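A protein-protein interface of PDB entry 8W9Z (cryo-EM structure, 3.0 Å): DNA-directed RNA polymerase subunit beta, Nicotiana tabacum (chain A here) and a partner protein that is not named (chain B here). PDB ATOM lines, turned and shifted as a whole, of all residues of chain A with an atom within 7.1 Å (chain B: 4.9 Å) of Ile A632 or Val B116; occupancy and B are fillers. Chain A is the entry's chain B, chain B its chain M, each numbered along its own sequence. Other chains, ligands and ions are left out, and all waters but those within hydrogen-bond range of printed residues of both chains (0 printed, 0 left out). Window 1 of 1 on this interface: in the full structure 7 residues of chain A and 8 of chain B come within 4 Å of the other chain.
Hydrophobic or aromatic side chains of chain B within 4 Å of the printed part of chain A: Leu B71, Met B113 and Val B116. Printed residues of chain A that touch a printed residue of chain B: Glu A584, Arg A586, Cys A631, Ile A632 and Lys A633. Among the printed residues, 9 pairs touch across the chains. Among the printed residues, Asp or Glu carboxylates within 4 Å of a Lys or Arg side-chain nitrogen of the other chain: Arg A586 with Glu B119 and Lys A633 with Glu B112.
Among the printed residues, pairs that only touch across the chains: Glu A584 with Leu B71, Cys A631 with Val B116, Cys A631 with Glu B117, Ile A632 with Val B116, Lys A633 with Met B113 and Lys A633 with Val B116.
The backbone carbonyl oxygen of Glu B117 lies within hydrogen-bond range of the guanidinium group of Arg A586. The side-chain carboxylate of Glu B119 is in salt-bridge range of the guanidinium group of Arg A586 (3.5 Å). The side-chain amino group of Lys A633 is in salt-bridge range of the side-chain carboxylate of Glu B112 (3.5 Å).
Ile A632 touches just one residue of chain B: Val B116. Of chain A, only Cys A631 (3.9 Å), Ile A632 (3.5 Å) and Lys A633 (3.9 Å) come within 4 Å of Val B116. Of the printed residues of chain B, Cys A631 touches Val B116 (3.9 Å) and Glu B117 (3.6 Å). Of the printed residues of chain A, Glu B117 touches Arg A586 (2.6 Å) and Cys A631 (3.6 Å). Of the printed residues of chain A, Leu B71 touches Glu A584. Of the printed residues of chain A, Glu B119 touches Arg A586 (3.5 Å). Of the printed residues of chain B, Glu A584 touches Leu B71 (3.99 Å). The nearest printed residue of chain B that does not touch Ile A632 is Met B113 (5.1 Å). The nearest printed residue of chain A that does not touch Leu B71 is Lys A633 (6.4 Å).
The guanidinium group of Arg A586 lies close to the side-chain sulfur of Cys A631. N of Ile A632 is in hydrogen-bond range of O of Gly A585, at 3.1 Å.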
ATOM      1  N   ALA A 581      22.829  28.824 -10.770  1.00  0.00           N
ATOM      2  CA  ALA A 581      24.074  28.665 -10.033  1.00  0.00           C
ATOM      3  C   ALA A 581      24.715  27.322 -10.356  1.00  0.00           C
ATOM      4  O   ALA A 581      24.054  26.280 -10.313  1.00  0.00           O
ATOM      5  CB  ALA A 581      23.822  28.784  -8.531  1.00  0.00           C
ATOM      6  N   GLU A 582      26.006  27.352 -10.682  1.00  0.00           N
ATOM      7  CA  GLU A 582      26.786  26.147 -10.925  1.00  0.00           C
ATOM      8  C   GLU A 582      27.566  25.704  -9.695  1.00  0.00           C
ATOM      9  O   GLU A 582      28.345  24.750  -9.776  1.00  0.00           O
ATOM     10  CB  GLU A 582      27.741  26.372 -12.104  1.00  0.00           C
ATOM     11  CG  GLU A 582      28.160  25.103 -12.839  1.00  0.00           C
ATOM     12  CD  GLU A 582      27.010  24.445 -13.577  1.00  0.00           C
ATOM     13  OE1 GLU A 582      26.023  25.141 -13.895  1.00  0.00           O
ATOM     14  OE2 GLU A 582      27.093  23.226 -13.842  1.00  0.00           O
ATOM     15  N   ARG A 583      27.371  26.370  -8.561  1.00  0.00           N
ATOM     16  CA  ARG A 583      28.070  26.030  -7.331  1.00  0.00           C
ATOM     17  C   ARG A 583      27.249  26.550  -6.161  1.00  0.00           C
ATOM     18  O   ARG A 583      26.365  27.394  -6.327  1.00  0.00           O
ATOM     19  CB  ARG A 583      29.486  26.617  -7.313  1.00  0.00           C
ATOM     20  CG  ARG A 583      30.450  25.922  -6.366  1.00  0.00           C
ATOM     21  CD  ARG A 583      31.786  26.644  -6.325  1.00  0.00           C
ATOM     22  NE  ARG A 583      32.324  26.868  -7.663  1.00  0.00           N
ATOM     23  CZ  ARG A 583      33.118  26.015  -8.301  1.00  0.00           C
ATOM     24  NH1 ARG A 583      33.470  24.874  -7.724  1.00  0.00           N
ATOM     25  NH2 ARG A 583      33.561  26.302  -9.517  1.00  0.00           N
ATOM     26  N   GLU A 584      27.549  26.033  -4.975  1.00  0.00           N
ATOM     27  CA  GLU A 584      26.864  26.430  -3.755  1.00  0.00           C
ATOM     28  C   GLU A 584      27.739  27.382  -2.953  1.00  0.00           C
ATOM     29  O   GLU A 584      28.956  27.195  -2.857  1.00  0.00           O
ATOM     30  CB  GLU A 584      26.496  25.210  -2.906  1.00  0.00           C
ATOM     31  CG  GLU A 584      27.667  24.313  -2.524  1.00  0.00           C
ATOM     32  CD  GLU A 584      28.053  23.346  -3.627  1.00  0.00           C
ATOM     33  OE1 GLU A 584      27.336  23.289  -4.649  1.00  0.00           O
ATOM     34  OE2 GLU A 584      29.072  22.642  -3.471  1.00  0.00           O
ATOM     35  N   GLY A 585      27.119  28.405  -2.387  1.00  0.00           N
ATOM     36  CA  GLY A 585      27.846  29.369  -1.589  1.00  0.00           C
ATOM     37  C   GLY A 585      27.042  30.636  -1.401  1.00  0.00           C
ATOM     38  O   GLY A 585      25.920  30.771  -1.888  1.00  0.00           O
ATOM     39  N   ARG A 586      27.650  31.567  -0.674  1.00  0.00           N
ATOM     40  CA  ARG A 586      27.041  32.859  -0.403  1.00  0.00           C
ATOM     41  C   ARG A 586      27.399  33.860  -1.494  1.00  0.00           C
ATOM     42  O   ARG A 586      28.460  33.777  -2.118  1.00  0.00           O
ATOM     43  CB  ARG A 586      27.485  33.395   0.958  1.00  0.00           C
ATOM     44  CG  ARG A 586      27.026  32.556   2.136  1.00  0.00           C
ATOM     45  CD  ARG A 586      27.421  33.196   3.454  1.00  0.00           C
ATOM     46  NE  ARG A 586      26.927  32.436   4.599  1.00  0.00           N
ATOM     47  CZ  ARG A 586      27.602  31.459   5.195  1.00  0.00           C
ATOM     48  NH1 ARG A 586      28.806  31.119   4.755  1.00  0.00           N
ATOM     49  NH2 ARG A 586      27.074  30.821   6.230  1.00  0.00           N
ATOM     50  N   VAL A 587      26.498  34.811  -1.717  1.00  0.00           N
ATOM     51  CA  VAL A 587      26.709  35.874  -2.693  1.00  0.00           C
ATOM     52  C   VAL A 587      27.378  37.038  -1.970  1.00  0.00           C
ATOM     53  O   VAL A 587      26.738  37.746  -1.190  1.00  0.00           O
ATOM     54  CB  VAL A 587      25.392  36.305  -3.350  1.00  0.00           C
ATOM     55  CG1 VAL A 587      25.666  37.260  -4.497  1.00  0.00           C
ATOM     56  CG2 VAL A 587      24.622  35.089  -3.835  1.00  0.00           C
ATOM     57  N   LEU A 597      30.082  34.675  -6.605  1.00  0.00           N
ATOM     58  CA  LEU A 597      29.614  33.605  -5.734  1.00  0.00           C
ATOM     59  C   LEU A 597      30.821  32.949  -5.079  1.00  0.00           C
ATOM     60  O   LEU A 597      31.701  32.427  -5.774  1.00  0.00           O
ATOM     61  CB  LEU A 597      28.795  32.581  -6.520  1.00  0.00           C
ATOM     62  CG  LEU A 597      28.117  31.471  -5.719  1.00  0.00           C
ATOM     63  CD1 LEU A 597      27.145  32.059  -4.711  1.00  0.00           C
ATOM     64  CD2 LEU A 597      27.407  30.505  -6.652  1.00  0.00           C
ATOM     65  N   VAL A 626      18.516  37.870  -6.066  1.00  0.00           N
ATOM     66  CA  VAL A 626      19.036  37.396  -4.790  1.00  0.00           C
ATOM     67  C   VAL A 626      19.799  38.540  -4.137  1.00  0.00           C
ATOM     68  O   VAL A 626      20.643  39.159  -4.787  1.00  0.00           O
ATOM     69  CB  VAL A 626      19.943  36.161  -4.940  1.00  0.00           C
ATOM     70  CG1 VAL A 626      19.103  34.925  -5.223  1.00  0.00           C
ATOM     71  CG2 VAL A 626      20.965  36.369  -6.048  1.00  0.00           C
ATOM     72  N   LYS A 630      23.299  35.905   0.960  1.00  0.00           N
ATOM     73  CA  LYS A 630      22.415  34.767   1.155  1.00  0.00           C
ATOM     74  C   LYS A 630      23.020  33.519   0.528  1.00  0.00           C
ATOM     75  O   LYS A 630      23.832  33.590  -0.399  1.00  0.00           O
ATOM     76  CB  LYS A 630      21.028  35.032   0.560  1.00  0.00           C
ATOM     77  CG  LYS A 630      20.999  35.075  -0.956  1.00  0.00           C
ATOM     78  CD  LYS A 630      19.572  35.123  -1.472  1.00  0.00           C
ATOM     79  CE  LYS A 630      18.785  33.896  -1.042  1.00  0.00           C
ATOM     80  NZ  LYS A 630      17.384  33.933  -1.544  1.00  0.00           N
ATOM     81  N   CYS A 631      22.611  32.367   1.047  1.00  0.00           N
ATOM     82  CA  CYS A 631      23.113  31.087   0.575  1.00  0.00           C
ATOM     83  C   CYS A 631      22.314  30.607  -0.631  1.00  0.00           C
ATOM     84  O   CYS A 631      21.121  30.890  -0.764  1.00  0.00           O
ATOM     85  CB  CYS A 631      23.060  30.043   1.689  1.00  0.00           C
ATOM     86  SG  CYS A 631      24.084  30.444   3.123  1.00  0.00           S
ATOM     87  N   ILE A 632      22.991  29.870  -1.512  1.00  0.00           N
ATOM     88  CA  ILE A 632      22.391  29.357  -2.736  1.00  0.00           C
ATOM     89  C   ILE A 632      22.883  27.933  -2.958  1.00  0.00           C
ATOM     90  O   ILE A 632      23.911  27.512  -2.424  1.00  0.00           O
ATOM     91  CB  ILE A 632      22.722  30.246  -3.959  1.00  0.00           C
ATOM     92  CG1 ILE A 632      21.628  30.137  -5.024  1.00  0.00           C
ATOM     93  CG2 ILE A 632      24.078  29.883  -4.543  1.00  0.00           C
ATOM     94  CD1 ILE A 632      20.333  30.810  -4.634  1.00  0.00           C
ATOM     95  N   LYS A 633      22.122  27.184  -3.750  1.00  0.00           N
ATOM     96  CA  LYS A 633      22.471  25.826  -4.136  1.00  0.00           C
ATOM     97  C   LYS A 633      22.566  25.735  -5.653  1.00  0.00           C
ATOM     98  O   LYS A 633      22.114  26.621  -6.382  1.00  0.00           O
ATOM     99  CB  LYS A 633      21.445  24.815  -3.607  1.00  0.00           C
ATOM    100  CG  LYS A 633      21.403  24.702  -2.096  1.00  0.00           C
ATOM    101  CD  LYS A 633      20.544  23.530  -1.656  1.00  0.00           C
ATOM    102  CE  LYS A 633      19.109  23.684  -2.129  1.00  0.00           C
ATOM    103  NZ  LYS A 633      18.253  22.552  -1.682  1.00  0.00           N
ATOM    104  N   LYS A 634      23.165  24.647  -6.129  1.00  0.00           N
ATOM    105  CA  LYS A 634      23.287  24.438  -7.564  1.00  0.00           C
ATOM    106  C   LYS A 634      21.915  24.208  -8.181  1.00  0.00           C
ATOM    107  O   LYS A 634      21.179  23.309  -7.766  1.00  0.00           O
ATOM    108  CB  LYS A 634      24.200  23.251  -7.864  1.00  0.00           C
ATOM    109  CG  LYS A 634      24.111  22.783  -9.308  1.00  0.00           C
ATOM    110  CD  LYS A 634      25.039  21.620  -9.596  1.00  0.00           C
ATOM    111  CE  LYS A 634      26.489  22.057  -9.594  1.00  0.00           C
ATOM    112  NZ  LYS A 634      27.377  20.978 -10.102  1.00  0.00           N
ATOM    113  N   GLY A 635      21.574  25.020  -9.176  1.00  0.00           N
ATOM    114  CA  GLY A 635      20.299  24.916  -9.850  1.00  0.00           C
ATOM    115  C   GLY A 635      19.279  25.959  -9.461  1.00  0.00           C
ATOM    116  O   GLY A 635      18.177  25.959 -10.023  1.00  0.00           O
ATOM    117  N   GLN A 636      19.603  26.845  -8.527  1.00  0.00           N
ATOM    118  CA  GLN A 636      18.698  27.904  -8.108  1.00  0.00           C
ATOM    119  C   GLN A 636      19.048  29.210  -8.809  1.00  0.00           C
ATOM    120  O   GLN A 636      20.193  29.436  -9.211  1.00  0.00           O
ATOM    121  CB  GLN A 636      18.737  28.089  -6.590  1.00  0.00           C
ATOM    122  CG  GLN A 636      18.239  26.881  -5.819  1.00  0.00           C
ATOM    123  CD  GLN A 636      18.005  27.174  -4.353  1.00  0.00           C
ATOM    124  OE1 GLN A 636      17.699  26.275  -3.572  1.00  0.00           O
ATOM    125  NE2 GLN A 636      18.140  28.436  -3.973  1.00  0.00           N
ATOM    126  N   ILE A 637      18.045  30.070  -8.950  1.00  0.00           N
ATOM    127  CA  ILE A 637      18.173  31.281  -9.752  1.00  0.00           C
ATOM    128  C   ILE A 637      18.999  32.314  -8.999  1.00  0.00           C
ATOM    129  O   ILE A 637      18.724  32.621  -7.834  1.00  0.00           O
ATOM    130  CB  ILE A 637      16.788  31.840 -10.114  1.00  0.00           C
ATOM    131  CG1 ILE A 637      16.044  30.861 -11.018  1.00  0.00           C
ATOM    132  CG2 ILE A 637      16.916  33.196 -10.788  1.00  0.00           C
ATOM    133  CD1 ILE A 637      16.804  30.496 -12.273  1.00  0.00           C
ATOM    134  N   LEU A 638      20.016  32.853  -9.669  1.00  0.00           N
ATOM    135  CA  LEU A 638      20.774  33.995  -9.176  1.00  0.00           C
ATOM    136  C   LEU A 638      20.364  35.298  -9.844  1.00  0.00           C
ATOM    137  O   LEU A 638      20.344  36.345  -9.192  1.00  0.00           O
ATOM    138  CB  LEU A 638      22.275  33.772  -9.381  1.00  0.00           C
ATOM    139  CG  LEU A 638      22.944  32.755  -8.458  1.00  0.00           C
ATOM    140  CD1 LEU A 638      24.426  32.644  -8.770  1.00  0.00           C
ATOM    141  CD2 LEU A 638      22.729  33.134  -7.002  1.00  0.00           C
ATOM    142  N   LEU B  71      25.076  17.305  -1.113  1.00  0.00           N
ATOM    143  CA  LEU B  71      26.190  17.476  -0.192  1.00  0.00           C
ATOM    144  C   LEU B  71      26.106  16.628   1.067  1.00  0.00           C
ATOM    145  O   LEU B  71      27.132  16.445   1.729  1.00  0.00           O
ATOM    146  CB  LEU B  71      26.326  18.951   0.225  1.00  0.00           C
ATOM    147  CG  LEU B  71      26.965  19.932  -0.762  1.00  0.00           C
ATOM    148  CD1 LEU B  71      26.028  20.268  -1.914  1.00  0.00           C
ATOM    149  CD2 LEU B  71      27.405  21.197  -0.042  1.00  0.00           C
ATOM    150  N   GLU B 112      19.981  20.160   3.382  1.00  0.00           N
ATOM    151  CA  GLU B 112      20.936  20.632   2.384  1.00  0.00           C
ATOM    152  C   GLU B 112      21.200  22.125   2.531  1.00  0.00           C
ATOM    153  O   GLU B 112      22.347  22.573   2.409  1.00  0.00           O
ATOM    154  CB  GLU B 112      20.435  20.312   0.978  1.00  0.00           C
ATOM    155  CG  GLU B 112      20.575  18.855   0.597  1.00  0.00           C
ATOM    156  CD  GLU B 112      20.223  18.600  -0.851  1.00  0.00           C
ATOM    157  OE1 GLU B 112      19.248  19.203  -1.345  1.00  0.00           O
ATOM    158  OE2 GLU B 112      20.933  17.804  -1.497  1.00  0.00           O
ATOM    159  N   MET B 113      20.156  22.915   2.794  1.00  0.00           N
ATOM    160  CA  MET B 113      20.371  24.337   3.037  1.00  0.00           C
ATOM    161  C   MET B 113      21.221  24.568   4.281  1.00  0.00           C
ATOM    162  O   MET B 113      22.091  25.447   4.282  1.00  0.00           O
ATOM    163  CB  MET B 113      19.033  25.062   3.166  1.00  0.00           C
ATOM    164  CG  MET B 113      18.268  25.180   1.859  1.00  0.00           C
ATOM    165  SD  MET B 113      19.196  26.101   0.617  1.00  0.00           S
ATOM    166  CE  MET B 113      19.436  27.659   1.463  1.00  0.00           C
ATOM    167  N   LEU B 114      20.996  23.782   5.337  1.00  0.00           N
ATOM    168  CA  LEU B 114      21.795  23.928   6.548  1.00  0.00           C
ATOM    169  C   LEU B 114      23.241  23.506   6.318  1.00  0.00           C
ATOM    170  O   LEU B 114      24.154  24.063   6.938  1.00  0.00           O
ATOM    171  CB  LEU B 114      21.173  23.115   7.682  1.00  0.00           C
ATOM    172  CG  LEU B 114      21.710  23.358   9.092  1.00  0.00           C
ATOM    173  CD1 LEU B 114      21.498  24.804   9.499  1.00  0.00           C
ATOM    174  CD2 LEU B 114      21.042  22.417  10.079  1.00  0.00           C
ATOM    175  N   ALA B 115      23.467  22.531   5.436  1.00  0.00           N
ATOM    176  CA  ALA B 115      24.831  22.138   5.104  1.00  0.00           C
ATOM    177  C   ALA B 115      25.517  23.184   4.234  1.00  0.00           C
ATOM    178  O   ALA B 115      26.738  23.352   4.315  1.00  0.00           O
ATOM    179  CB  ALA B 115      24.834  20.780   4.404  1.00  0.00           C
ATOM    180  N   VAL B 116      24.753  23.884   3.396  1.00  0.00           N
ATOM    181  CA  VAL B 116      25.324  24.973   2.610  1.00  0.00           C
ATOM    182  C   VAL B 116      25.666  26.158   3.507  1.00  0.00           C
ATOM    183  O   VAL B 116      26.682  26.832   3.303  1.00  0.00           O
ATOM    184  CB  VAL B 116      24.360  25.370   1.476  1.00  0.00           C
ATOM    185  CG1 VAL B 116      24.827  26.643   0.791  1.00  0.00           C
ATOM    186  CG2 VAL B 116      24.249  24.244   0.465  1.00  0.00           C
ATOM    187  N   GLU B 117      24.837  26.423   4.521  1.00  0.00           N
ATOM    188  CA  GLU B 117      25.125  27.523   5.438  1.00  0.00           C
ATOM    189  C   GLU B 117      26.379  27.263   6.263  1.00  0.00           C
ATOM    190  O   GLU B 117      27.149  28.195   6.525  1.00  0.00           O
ATOM    191  CB  GLU B 117      23.929  27.772   6.357  1.00  0.00           C
ATOM    192  CG  GLU B 117      22.693  28.283   5.639  1.00  0.00           C
ATOM    193  CD  GLU B 117      21.536  28.544   6.580  1.00  0.00           C
ATOM    194  OE1 GLU B 117      21.745  28.502   7.811  1.00  0.00           O
ATOM    195  OE2 GLU B 117      20.413  28.791   6.089  1.00  0.00           O
ATOM    196  N   TYR B 118      26.604  26.020   6.678  1.00  0.00           N
ATOM    197  CA  TYR B 118      27.789  25.630   7.441  1.00  0.00           C
ATOM    198  C   TYR B 118      28.629  24.719   6.548  1.00  0.00           C
ATOM    199  O   TYR B 118      28.458  23.500   6.545  1.00  0.00           O
ATOM    200  CB  TYR B 118      27.404  24.931   8.742  1.00  0.00           C
ATOM    201  CG  TYR B 118      26.583  25.777   9.686  1.00  0.00           C
ATOM    202  CD1 TYR B 118      27.196  26.608  10.613  1.00  0.00           C
ATOM    203  CD2 TYR B 118      25.197  25.736   9.660  1.00  0.00           C
ATOM    204  CE1 TYR B 118      26.450  27.380  11.481  1.00  0.00           C
ATOM    205  CE2 TYR B 118      24.444  26.505  10.524  1.00  0.00           C
ATOM    206  CZ  TYR B 118      25.075  27.325  11.432  1.00  0.00           C
ATOM    207  OH  TYR B 118      24.328  28.092  12.295  1.00  0.00           O
ATOM    208  N   GLU B 119      29.547  25.323   5.790  1.00  0.00           N
ATOM    209  CA  GLU B 119      30.323  24.551   4.824  1.00  0.00           C
ATOM    210  C   GLU B 119      31.348  23.660   5.515  1.00  0.00           C
ATOM    211  O   GLU B 119      31.589  22.528   5.078  1.00  0.00           O
ATOM    212  CB  GLU B 119      31.003  25.486   3.821  1.00  0.00           C
ATOM    213  CG  GLU B 119      31.955  26.513   4.428  1.00  0.00           C
ATOM    214  CD  GLU B 119      31.238  27.728   4.987  1.00  0.00           C
ATOM    215  OE1 GLU B 119      30.001  27.819   4.829  1.00  0.00           O
ATOM    216  OE2 GLU B 119      31.912  28.595   5.583  1.00  0.00           O
